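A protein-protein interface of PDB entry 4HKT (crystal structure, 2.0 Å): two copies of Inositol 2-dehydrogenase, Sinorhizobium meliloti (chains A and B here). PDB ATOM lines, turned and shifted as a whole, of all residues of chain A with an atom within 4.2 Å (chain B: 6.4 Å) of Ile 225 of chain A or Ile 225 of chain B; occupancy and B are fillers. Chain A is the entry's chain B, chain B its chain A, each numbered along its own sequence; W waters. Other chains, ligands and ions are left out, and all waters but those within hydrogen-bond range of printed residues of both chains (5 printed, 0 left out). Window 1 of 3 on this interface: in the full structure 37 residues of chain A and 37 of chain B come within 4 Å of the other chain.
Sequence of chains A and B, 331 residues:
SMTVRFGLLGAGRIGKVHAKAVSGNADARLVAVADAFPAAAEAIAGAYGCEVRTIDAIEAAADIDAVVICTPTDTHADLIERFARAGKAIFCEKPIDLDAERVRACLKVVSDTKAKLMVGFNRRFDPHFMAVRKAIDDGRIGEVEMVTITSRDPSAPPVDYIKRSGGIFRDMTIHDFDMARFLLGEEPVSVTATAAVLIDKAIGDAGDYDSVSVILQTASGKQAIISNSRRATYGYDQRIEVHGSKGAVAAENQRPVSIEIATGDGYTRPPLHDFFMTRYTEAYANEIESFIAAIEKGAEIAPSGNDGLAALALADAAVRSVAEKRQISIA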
ATOM      1  N   VAL A 147       4.792  16.777 -25.052  1.00  0.00           N
ATOM      2  CA  VAL A 147       3.991  16.204 -23.970  1.00  0.00           C
ATOM      3  C   VAL A 147       3.926  14.713 -24.207  1.00  0.00           C
ATOM      4  O   VAL A 147       3.796  14.276 -25.357  1.00  0.00           O
ATOM      5  CB  VAL A 147       2.553  16.771 -24.012  1.00  0.00           C
ATOM      6  CG1 VAL A 147       1.616  16.027 -23.059  1.00  0.00           C
ATOM      7  CG2 VAL A 147       2.589  18.251 -23.713  1.00  0.00           C
ATOM      8  N   THR A 148       4.032  13.925 -23.147  1.00  0.00           N
ATOM      9  CA  THR A 148       3.847  12.488 -23.230  1.00  0.00           C
ATOM     10  C   THR A 148       2.846  12.052 -22.141  1.00  0.00           C
ATOM     11  O   THR A 148       2.957  12.432 -20.940  1.00  0.00           O
ATOM     12  CB  THR A 148       5.164  11.692 -23.072  1.00  0.00           C
ATOM     13  OG1 THR A 148       6.191  12.278 -23.874  1.00  0.00           O
ATOM     14  CG2 THR A 148       4.991  10.230 -23.534  1.00  0.00           C
ATOM     15  N   ILE A 149       1.852  11.314 -22.585  1.00  0.00           N
ATOM     16  CA  ILE A 149       0.703  10.907 -21.752  1.00  0.00           C
ATOM     17  C   ILE A 149       0.564   9.419 -21.941  1.00  0.00           C
ATOM     18  O   ILE A 149       0.434   8.950 -23.068  1.00  0.00           O
ATOM     19  CB  ILE A 149      -0.595  11.608 -22.178  1.00  0.00           C
ATOM     20  CG1 ILE A 149      -0.521  13.097 -21.953  1.00  0.00           C
ATOM     21  CG2 ILE A 149      -1.836  11.066 -21.436  1.00  0.00           C
ATOM     22  CD1 ILE A 149      -1.619  13.852 -22.660  1.00  0.00           C
ATOM     23  N   SER A 213      -1.989   4.472 -30.105  1.00  0.00           N
ATOM     24  CA  SER A 213      -0.940   5.460 -29.985  1.00  0.00           C
ATOM     25  C   SER A 213      -1.387   6.658 -30.835  1.00  0.00           C
ATOM     26  O   SER A 213      -1.901   6.487 -31.949  1.00  0.00           O
ATOM     27  CB  SER A 213       0.355   4.931 -30.541  1.00  0.00           C
ATOM     28  OG  SER A 213       0.777   3.735 -29.948  1.00  0.00           O
ATOM     29  N   VAL A 214      -1.227   7.866 -30.294  1.00  0.00           N
ATOM     30  CA  VAL A 214      -1.670   9.087 -30.991  1.00  0.00           C
ATOM     31  C   VAL A 214      -0.601  10.177 -30.886  1.00  0.00           C
ATOM     32  O   VAL A 214       0.048  10.267 -29.893  1.00  0.00           O
ATOM     33  CB  VAL A 214      -2.968   9.631 -30.413  1.00  0.00           C
ATOM     34  CG1 VAL A 214      -3.485  10.767 -31.282  1.00  0.00           C
ATOM     35  CG2 VAL A 214      -4.041   8.565 -30.334  1.00  0.00           C
ATOM     36  N   ALA A 224       2.149  16.280 -28.741  1.00  0.00           N
ATOM     37  CA  ALA A 224       1.698  15.450 -27.636  1.00  0.00           C
ATOM     38  C   ALA A 224       1.558  14.043 -28.150  1.00  0.00           C
ATOM     39  O   ALA A 224       0.921  13.817 -29.129  1.00  0.00           O
ATOM     40  CB  ALA A 224       0.363  15.930 -27.082  1.00  0.00           C
ATOM     41  N   ILE A 225       2.220  13.120 -27.481  1.00  0.00           N
ATOM     42  CA  ILE A 225       2.109  11.743 -27.770  1.00  0.00           C
ATOM     43  C   ILE A 225       1.255  11.115 -26.685  1.00  0.00           C
ATOM     44  O   ILE A 225       1.463  11.354 -25.485  1.00  0.00           O
ATOM     45  CB  ILE A 225       3.490  11.091 -27.696  1.00  0.00           C
ATOM     46  CG1 ILE A 225       4.453  11.712 -28.677  1.00  0.00           C
ATOM     47  CG2 ILE A 225       3.402   9.622 -28.017  1.00  0.00           C
ATOM     48  CD1 ILE A 225       5.873  11.170 -28.547  1.00  0.00           C
ATOM     49  N   ILE A 226       0.327  10.272 -27.094  1.00  0.00           N
ATOM     50  CA  ILE A 226      -0.556   9.617 -26.152  1.00  0.00           C
ATOM     51  C   ILE A 226      -0.456   8.120 -26.431  1.00  0.00           C
ATOM     52  O   ILE A 226      -0.548   7.674 -27.582  1.00  0.00           O
ATOM     53  CB  ILE A 226      -2.017  10.027 -26.318  1.00  0.00           C
ATOM     54  CG1 ILE A 226      -2.240  11.472 -25.969  1.00  0.00           C
ATOM     55  CG2 ILE A 226      -2.918   9.117 -25.473  1.00  0.00           C
ATOM     56  CD1 ILE A 226      -3.472  12.006 -26.670  1.00  0.00           C
ATOM     57  N   SER A 227      -0.289   7.358 -25.367  1.00  0.00           N
ATOM     58  CA  SER A 227      -0.283   5.880 -25.409  1.00  0.00           C
ATOM     59  C   SER A 227      -1.423   5.338 -24.519  1.00  0.00           C
ATOM     60  O   SER A 227      -1.531   5.739 -23.366  1.00  0.00           O
ATOM     61  CB  SER A 227       1.047   5.428 -24.820  1.00  0.00           C
ATOM     62  OG  SER A 227       1.219   4.052 -24.824  1.00  0.00           O
ATOM     63  N   MET B 146       3.427  -2.695 -26.331  1.00  0.00           N
ATOM     64  CA  MET B 146       3.654  -1.263 -26.572  1.00  0.00           C
ATOM     65  C   MET B 146       5.002  -0.849 -26.041  1.00  0.00           C
ATOM     66  O   MET B 146       5.313  -1.022 -24.856  1.00  0.00           O
ATOM     67  CB  MET B 146       2.510  -0.420 -26.009  1.00  0.00           C
ATOM     68  CG  MET B 146       1.173  -0.932 -26.576  1.00  0.00           C
ATOM     69  SD  MET B 146      -0.368   0.197 -26.117  1.00  0.00           S
ATOM     70  CE  MET B 146       0.126   1.802 -27.116  1.00  0.00           C
ATOM     71  N   VAL B 147       5.806  -0.273 -26.919  1.00  0.00           N
ATOM     72  CA  VAL B 147       7.151   0.201 -26.592  1.00  0.00           C
ATOM     73  C   VAL B 147       7.130   1.749 -26.557  1.00  0.00           C
ATOM     74  O   VAL B 147       6.528   2.375 -27.423  1.00  0.00           O
ATOM     75  CB  VAL B 147       8.165  -0.323 -27.656  1.00  0.00           C
ATOM     76  CG1 VAL B 147       9.568   0.228 -27.422  1.00  0.00           C
ATOM     77  CG2 VAL B 147       8.205  -1.841 -27.648  1.00  0.00           C
ATOM     78  N   THR B 148       7.716   2.351 -25.529  1.00  0.00           N
ATOM     79  CA  THR B 148       7.913   3.815 -25.454  1.00  0.00           C
ATOM     80  C   THR B 148       9.392   4.145 -25.248  1.00  0.00           C
ATOM     81  O   THR B 148      10.038   3.661 -24.306  1.00  0.00           O
ATOM     82  CB  THR B 148       7.097   4.462 -24.315  1.00  0.00           C
ATOM     83  OG1 THR B 148       5.740   4.070 -24.407  1.00  0.00           O
ATOM     84  CG2 THR B 148       7.120   5.971 -24.428  1.00  0.00           C
ATOM     85  N   ILE B 149       9.938   4.957 -26.146  1.00  0.00           N
ATOM     86  CA  ILE B 149      11.346   5.342 -26.105  1.00  0.00           C
ATOM     87  C   ILE B 149      11.460   6.864 -26.094  1.00  0.00           C
ATOM     88  O   ILE B 149      10.859   7.511 -26.934  1.00  0.00           O
ATOM     89  CB  ILE B 149      12.081   4.766 -27.313  1.00  0.00           C
ATOM     90  CG1 ILE B 149      12.140   3.241 -27.238  1.00  0.00           C
ATOM     91  CG2 ILE B 149      13.504   5.291 -27.438  1.00  0.00           C
ATOM     92  CD1 ILE B 149      12.403   2.595 -28.621  1.00  0.00           C
ATOM     93  N   THR B 150      12.163   7.416 -25.099  1.00  0.00           N
ATOM     94  CA  THR B 150      12.435   8.841 -25.020  1.00  0.00           C
ATOM     95  C   THR B 150      13.938   9.116 -25.010  1.00  0.00           C
ATOM     96  O   THR B 150      14.673   8.588 -24.166  1.00  0.00           O
ATOM     97  CB  THR B 150      11.784   9.444 -23.773  1.00  0.00           C
ATOM     98  OG1 THR B 150      10.385   9.164 -23.814  1.00  0.00           O
ATOM     99  CG2 THR B 150      11.968  10.947 -23.744  1.00  0.00           C
ATOM    100  N   VAL B 212      10.870  15.819 -32.473  1.00  0.00           N
ATOM    101  CA  VAL B 212      10.146  14.868 -33.263  1.00  0.00           C
ATOM    102  C   VAL B 212       9.457  13.735 -32.483  1.00  0.00           C
ATOM    103  O   VAL B 212       9.913  13.305 -31.422  1.00  0.00           O
ATOM    104  CB  VAL B 212      11.028  14.301 -34.383  1.00  0.00           C
ATOM    105  CG1 VAL B 212      11.660  15.434 -35.196  1.00  0.00           C
ATOM    106  CG2 VAL B 212      12.106  13.362 -33.847  1.00  0.00           C
ATOM    107  N   SER B 213       8.338  13.295 -33.037  1.00  0.00           N
ATOM    108  CA  SER B 213       7.546  12.215 -32.485  1.00  0.00           C
ATOM    109  C   SER B 213       7.278  11.198 -33.565  1.00  0.00           C
ATOM    110  O   SER B 213       6.984  11.553 -34.703  1.00  0.00           O
ATOM    111  CB  SER B 213       6.218  12.744 -31.935  1.00  0.00           C
ATOM    112  OG  SER B 213       6.443  13.803 -31.051  1.00  0.00           O
ATOM    113  N   VAL B 214       7.397   9.907 -33.204  1.00  0.00           N
ATOM    114  CA  VAL B 214       7.222   8.825 -34.165  1.00  0.00           C
ATOM    115  C   VAL B 214       6.453   7.632 -33.578  1.00  0.00           C
ATOM    116  O   VAL B 214       6.646   7.264 -32.416  1.00  0.00           O
ATOM    117  CB  VAL B 214       8.548   8.237 -34.669  1.00  0.00           C
ATOM    118  CG1 VAL B 214       8.281   7.304 -35.827  1.00  0.00           C
ATOM    119  CG2 VAL B 214       9.537   9.277 -35.129  1.00  0.00           C
ATOM    120  N   ILE B 215       5.555   7.070 -34.372  1.00  0.00           N
ATOM    121  CA  ILE B 215       4.925   5.811 -34.060  1.00  0.00           C
ATOM    122  C   ILE B 215       5.281   4.773 -35.131  1.00  0.00           C
ATOM    123  O   ILE B 215       5.048   5.015 -36.322  1.00  0.00           O
ATOM    124  CB  ILE B 215       3.392   5.908 -33.998  1.00  0.00           C
ATOM    125  CG1 ILE B 215       2.921   6.939 -32.950  1.00  0.00           C
ATOM    126  CG2 ILE B 215       2.835   4.547 -33.599  1.00  0.00           C
ATOM    127  CD1 ILE B 215       1.469   7.366 -33.174  1.00  0.00           C
ATOM    128  N   LEU B 216       5.851   3.654 -34.702  1.00  0.00           N
ATOM    129  CA  LEU B 216       6.065   2.491 -35.546  1.00  0.00           C
ATOM    130  C   LEU B 216       5.063   1.416 -35.206  1.00  0.00           C
ATOM    131  O   LEU B 216       4.717   1.246 -34.027  1.00  0.00           O
ATOM    132  CB  LEU B 216       7.405   1.902 -35.268  1.00  0.00           C
ATOM    133  CG  LEU B 216       8.575   2.826 -35.229  1.00  0.00           C
ATOM    134  CD1 LEU B 216       9.775   2.062 -34.793  1.00  0.00           C
ATOM    135  CD2 LEU B 216       8.805   3.421 -36.580  1.00  0.00           C
ATOM    136  N   GLN B 223       3.106  -1.711 -31.241  1.00  0.00           N
ATOM    137  CA  GLN B 223       3.451  -0.314 -31.542  1.00  0.00           C
ATOM    138  C   GLN B 223       4.613   0.186 -30.705  1.00  0.00           C
ATOM    139  O   GLN B 223       4.755  -0.178 -29.550  1.00  0.00           O
ATOM    140  CB  GLN B 223       2.234   0.569 -31.320  1.00  0.00           C
ATOM    141  CG  GLN B 223       1.089   0.311 -32.285  1.00  0.00           C
ATOM    142  CD  GLN B 223      -0.288   0.601 -31.649  1.00  0.00           C
ATOM    143  OE1 GLN B 223      -0.635   1.744 -31.356  1.00  0.00           O
ATOM    144  NE2 GLN B 223      -1.085  -0.442 -31.497  1.00  0.00           N
ATOM    145  N   ALA B 224       5.486   1.015 -31.300  1.00  0.00           N
ATOM    146  CA  ALA B 224       6.531   1.663 -30.559  1.00  0.00           C
ATOM    147  C   ALA B 224       6.416   3.197 -30.795  1.00  0.00           C
ATOM    148  O   ALA B 224       6.246   3.636 -31.915  1.00  0.00           O
ATOM    149  CB  ALA B 224       7.885   1.152 -31.016  1.00  0.00           C
ATOM    150  N   ILE B 225       6.412   3.956 -29.716  1.00  0.00           N
ATOM    151  CA  ILE B 225       6.397   5.396 -29.770  1.00  0.00           C
ATOM    152  C   ILE B 225       7.764   5.893 -29.382  1.00  0.00           C
ATOM    153  O   ILE B 225       8.355   5.453 -28.385  1.00  0.00           O
ATOM    154  CB  ILE B 225       5.341   5.970 -28.842  1.00  0.00           C
ATOM    155  CG1 ILE B 225       3.943   5.534 -29.257  1.00  0.00           C
ATOM    156  CG2 ILE B 225       5.399   7.471 -28.880  1.00  0.00           C
ATOM    157  CD1 ILE B 225       2.927   5.777 -28.167  1.00  0.00           C
ATOM    158  N   ILE B 226       8.278   6.822 -30.188  1.00  0.00           N
ATOM    159  CA  ILE B 226       9.569   7.427 -29.981  1.00  0.00           C
ATOM    160  C   ILE B 226       9.405   8.956 -29.823  1.00  0.00           C
ATOM    161  O   ILE B 226       8.716   9.584 -30.628  1.00  0.00           O
ATOM    162  CB  ILE B 226      10.540   7.108 -31.143  1.00  0.00           C
ATOM    163  CG1 ILE B 226      10.864   5.618 -31.210  1.00  0.00           C
ATOM    164  CG2 ILE B 226      11.879   7.807 -30.898  1.00  0.00           C
ATOM    165  CD1 ILE B 226      11.397   5.169 -32.571  1.00  0.00           C
ATOM    166  N   SER B 227      10.025   9.518 -28.784  1.00  0.00           N
ATOM    167  CA  SER B 227      10.056  10.963 -28.550  1.00  0.00           C
ATOM    168  C   SER B 227      11.525  11.411 -28.539  1.00  0.00           C
ATOM    169  O   SER B 227      12.307  10.868 -27.781  1.00  0.00           O
ATOM    170  CB  SER B 227       9.447  11.271 -27.159  1.00  0.00           C
ATOM    171  OG  SER B 227       9.473  12.652 -26.844  1.00  0.00           O
ATOM    172  N   ASN B 228      11.882  12.417 -29.345  1.00  0.00           N
ATOM    173  CA  ASN B 228      13.265  12.927 -29.434  1.00  0.00           C
ATOM    174  C   ASN B 228      13.231  14.454 -29.323  1.00  0.00           C
ATOM    175  O   ASN B 228      12.403  15.114 -29.960  1.00  0.00           O
ATOM    176  CB  ASN B 228      13.873  12.598 -30.821  1.00  0.00           C
ATOM    177  CG  ASN B 228      14.448  11.189 -30.974  1.00  0.00           C
ATOM    178  OD1 ASN B 228      15.010  10.902 -32.041  1.00  0.00           O
ATOM    179  ND2 ASN B 228      14.277  10.283 -29.978  1.00  0.00           N
HETATM  180  O   HOH W   1       3.063   2.606 -28.375  1.00  0.00           O
HETATM  181  O   HOH W   2      -0.099   2.162 -23.474  1.00  0.00           O
HETATM  182  O   HOH W   3       8.513  10.743 -22.575  1.00  0.00           O
HETATM  183  O   HOH W   4       3.647   3.133 -25.522  1.00  0.00           O
HETATM  184  O   HOH W   5       7.052  13.538 -25.993  1.00  0.00           O
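The backbone NH (N) of Ser 227 of chain A sits at hydrogen-bond distance from the backbone carbonyl oxygen (O) of Ile 149 of chain A, at 2.9 Å.
The backbone carbonyl oxygen (O) of Val 147 of chain A lies within hydrogen-bond range of the backbone NH (N) of Ile 225 of chain A, at 2.9 Å.
O of Ile 225 of chain B is in hydrogen-bond range of N of Ile 149 of chain B, 2.8 Å away.
N of Val 147 of chain B lies within hydrogen-bond range of O of Gln 223 of chain B (2.8 Å).
The backbone NH of Ile 225 of chain B is in hydrogen-bond range of the backbone carbonyl oxygen of Val 147 of chain B (2.8 Å).
O of Val 214 of chain B lies within hydrogen-bond range of N of Ile 226 of chain B (2.8 Å).
Among the printed residues, merely in contact across the chains: Ser 213 of chain A with Met 146 of chain B, Ser 213 of chain A with Ile 215 of chain B, Ser 213 of chain A with Ile 225 of chain B, Val 214 of chain A with Ile 215 of chain B, Ile 225 of chain A with Ser 213 of chain B, Ile 225 of chain A with Ile 225 of chain B, Ile 225 of chain A with Ile 226 of chain B, Ile 225 of chain A with Ser 227 of chain B, Ser 227 of chain A with Met 146 of chain B and Ser 227 of chain A with Ile 225 of chain B.
Ile 149 of chain A touches none of the printed residues of chain B.
Of chain B, only Ser 213 (3.7 Å), Ile 225 (3.1 Å), Ile 226 (3.9 Å) and Ser 227 (3.8 Å) come within 4 Å of Ile 225 of chain A.
Val 212 of chain B touches none of the printed residues of chain A.
Of the printed residues of chain A, Ile 225 of chain B touches Ser 213, Ile 225 and Ser 227.
Of the printed residues of chain A, Ile 226 of chain B touches Ile 225.
Of the printed residues of chain A, Ser 227 of chain B touches Ile 225.
The nearest printed residue of chain A that does not touch Ile 225 of chain B is Ile 226 of chain A (4.002 Å).
The nearest printed residue of chain A that does not touch Ile 226 of chain B is Thr 148 of chain A (7.5 Å).
Of the 16 printed residues of chain B, 7 touch a printed residue of chain A.
Printed residues of chain B that touch a printed residue of chain A: Met 146, Ser 213, Ile 215, Gln 223, Ile 225, Ile 226 and Ser 227.
Of the 9 printed residues of chain A, 4 touch a printed residue of chain B.
Hydrophobic or aromatic side chains of chain A that line the printed part of chain B: Ile 225.
Among the printed residues, no Asp or Glu carboxylate lies within 4 Å of a Lys or Arg side-chain nitrogen of the other chain.
Ser 213 of chain A touches Ile 225 of chain B, and with the chains exchanged Ile 225 of chain A touches Ser 213 of chain B.
Ile 225 of chain B touches its own counterpart, Ile 225 of chain A.
Ile 225 of chain A touches Ile 226 of chain B, but with the chains exchanged Ile 226 of chain A does not touch Ile 225 of chain B (4.002 Å).
Ile 225 of chain A touches Ser 227 of chain B, and with the chains exchanged Ser 227 of chain A touches Ile 225 of chain B.
Positions printed for both chains: 147, 148, 149, 213, 214, 224, 225, 226 and 227.
Of the 11 pairs that touch across the chains among the printed residues, 5 have their exchanged pair printed and touching as well.
Water W4 bridges OG1 of Thr 148 of chain B and OG of Ser 227 of chain A.
Water W5 lies within hydrogen-bond range of OG1 of Thr 148 of chain A (2.6 Å), OG of Ser 227 of chain B (2.7 Å) and O of Val 147 of chain A (3.4 Å).
Water W2 bridges OG of Ser 227 of chain A and SD of Met 146 of chain B.
Water W3 lies within hydrogen-bond range of OG1 of Thr 150 of chain B (2.7 Å) and OG1 of Thr 148 of chain A (3.1 Å).
Water W1 lies within hydrogen-bond range of the side-chain hydroxyl (OG) of Ser 213 of chain A and the backbone carbonyl oxygen (O) of Gln 223 of chain B.
The side-chain hydroxyl of Ser 213 of chain A sits at hydrogen-bond distance from the side-chain amide oxygen of Gln 223 of chain B, at 2.8 Å.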
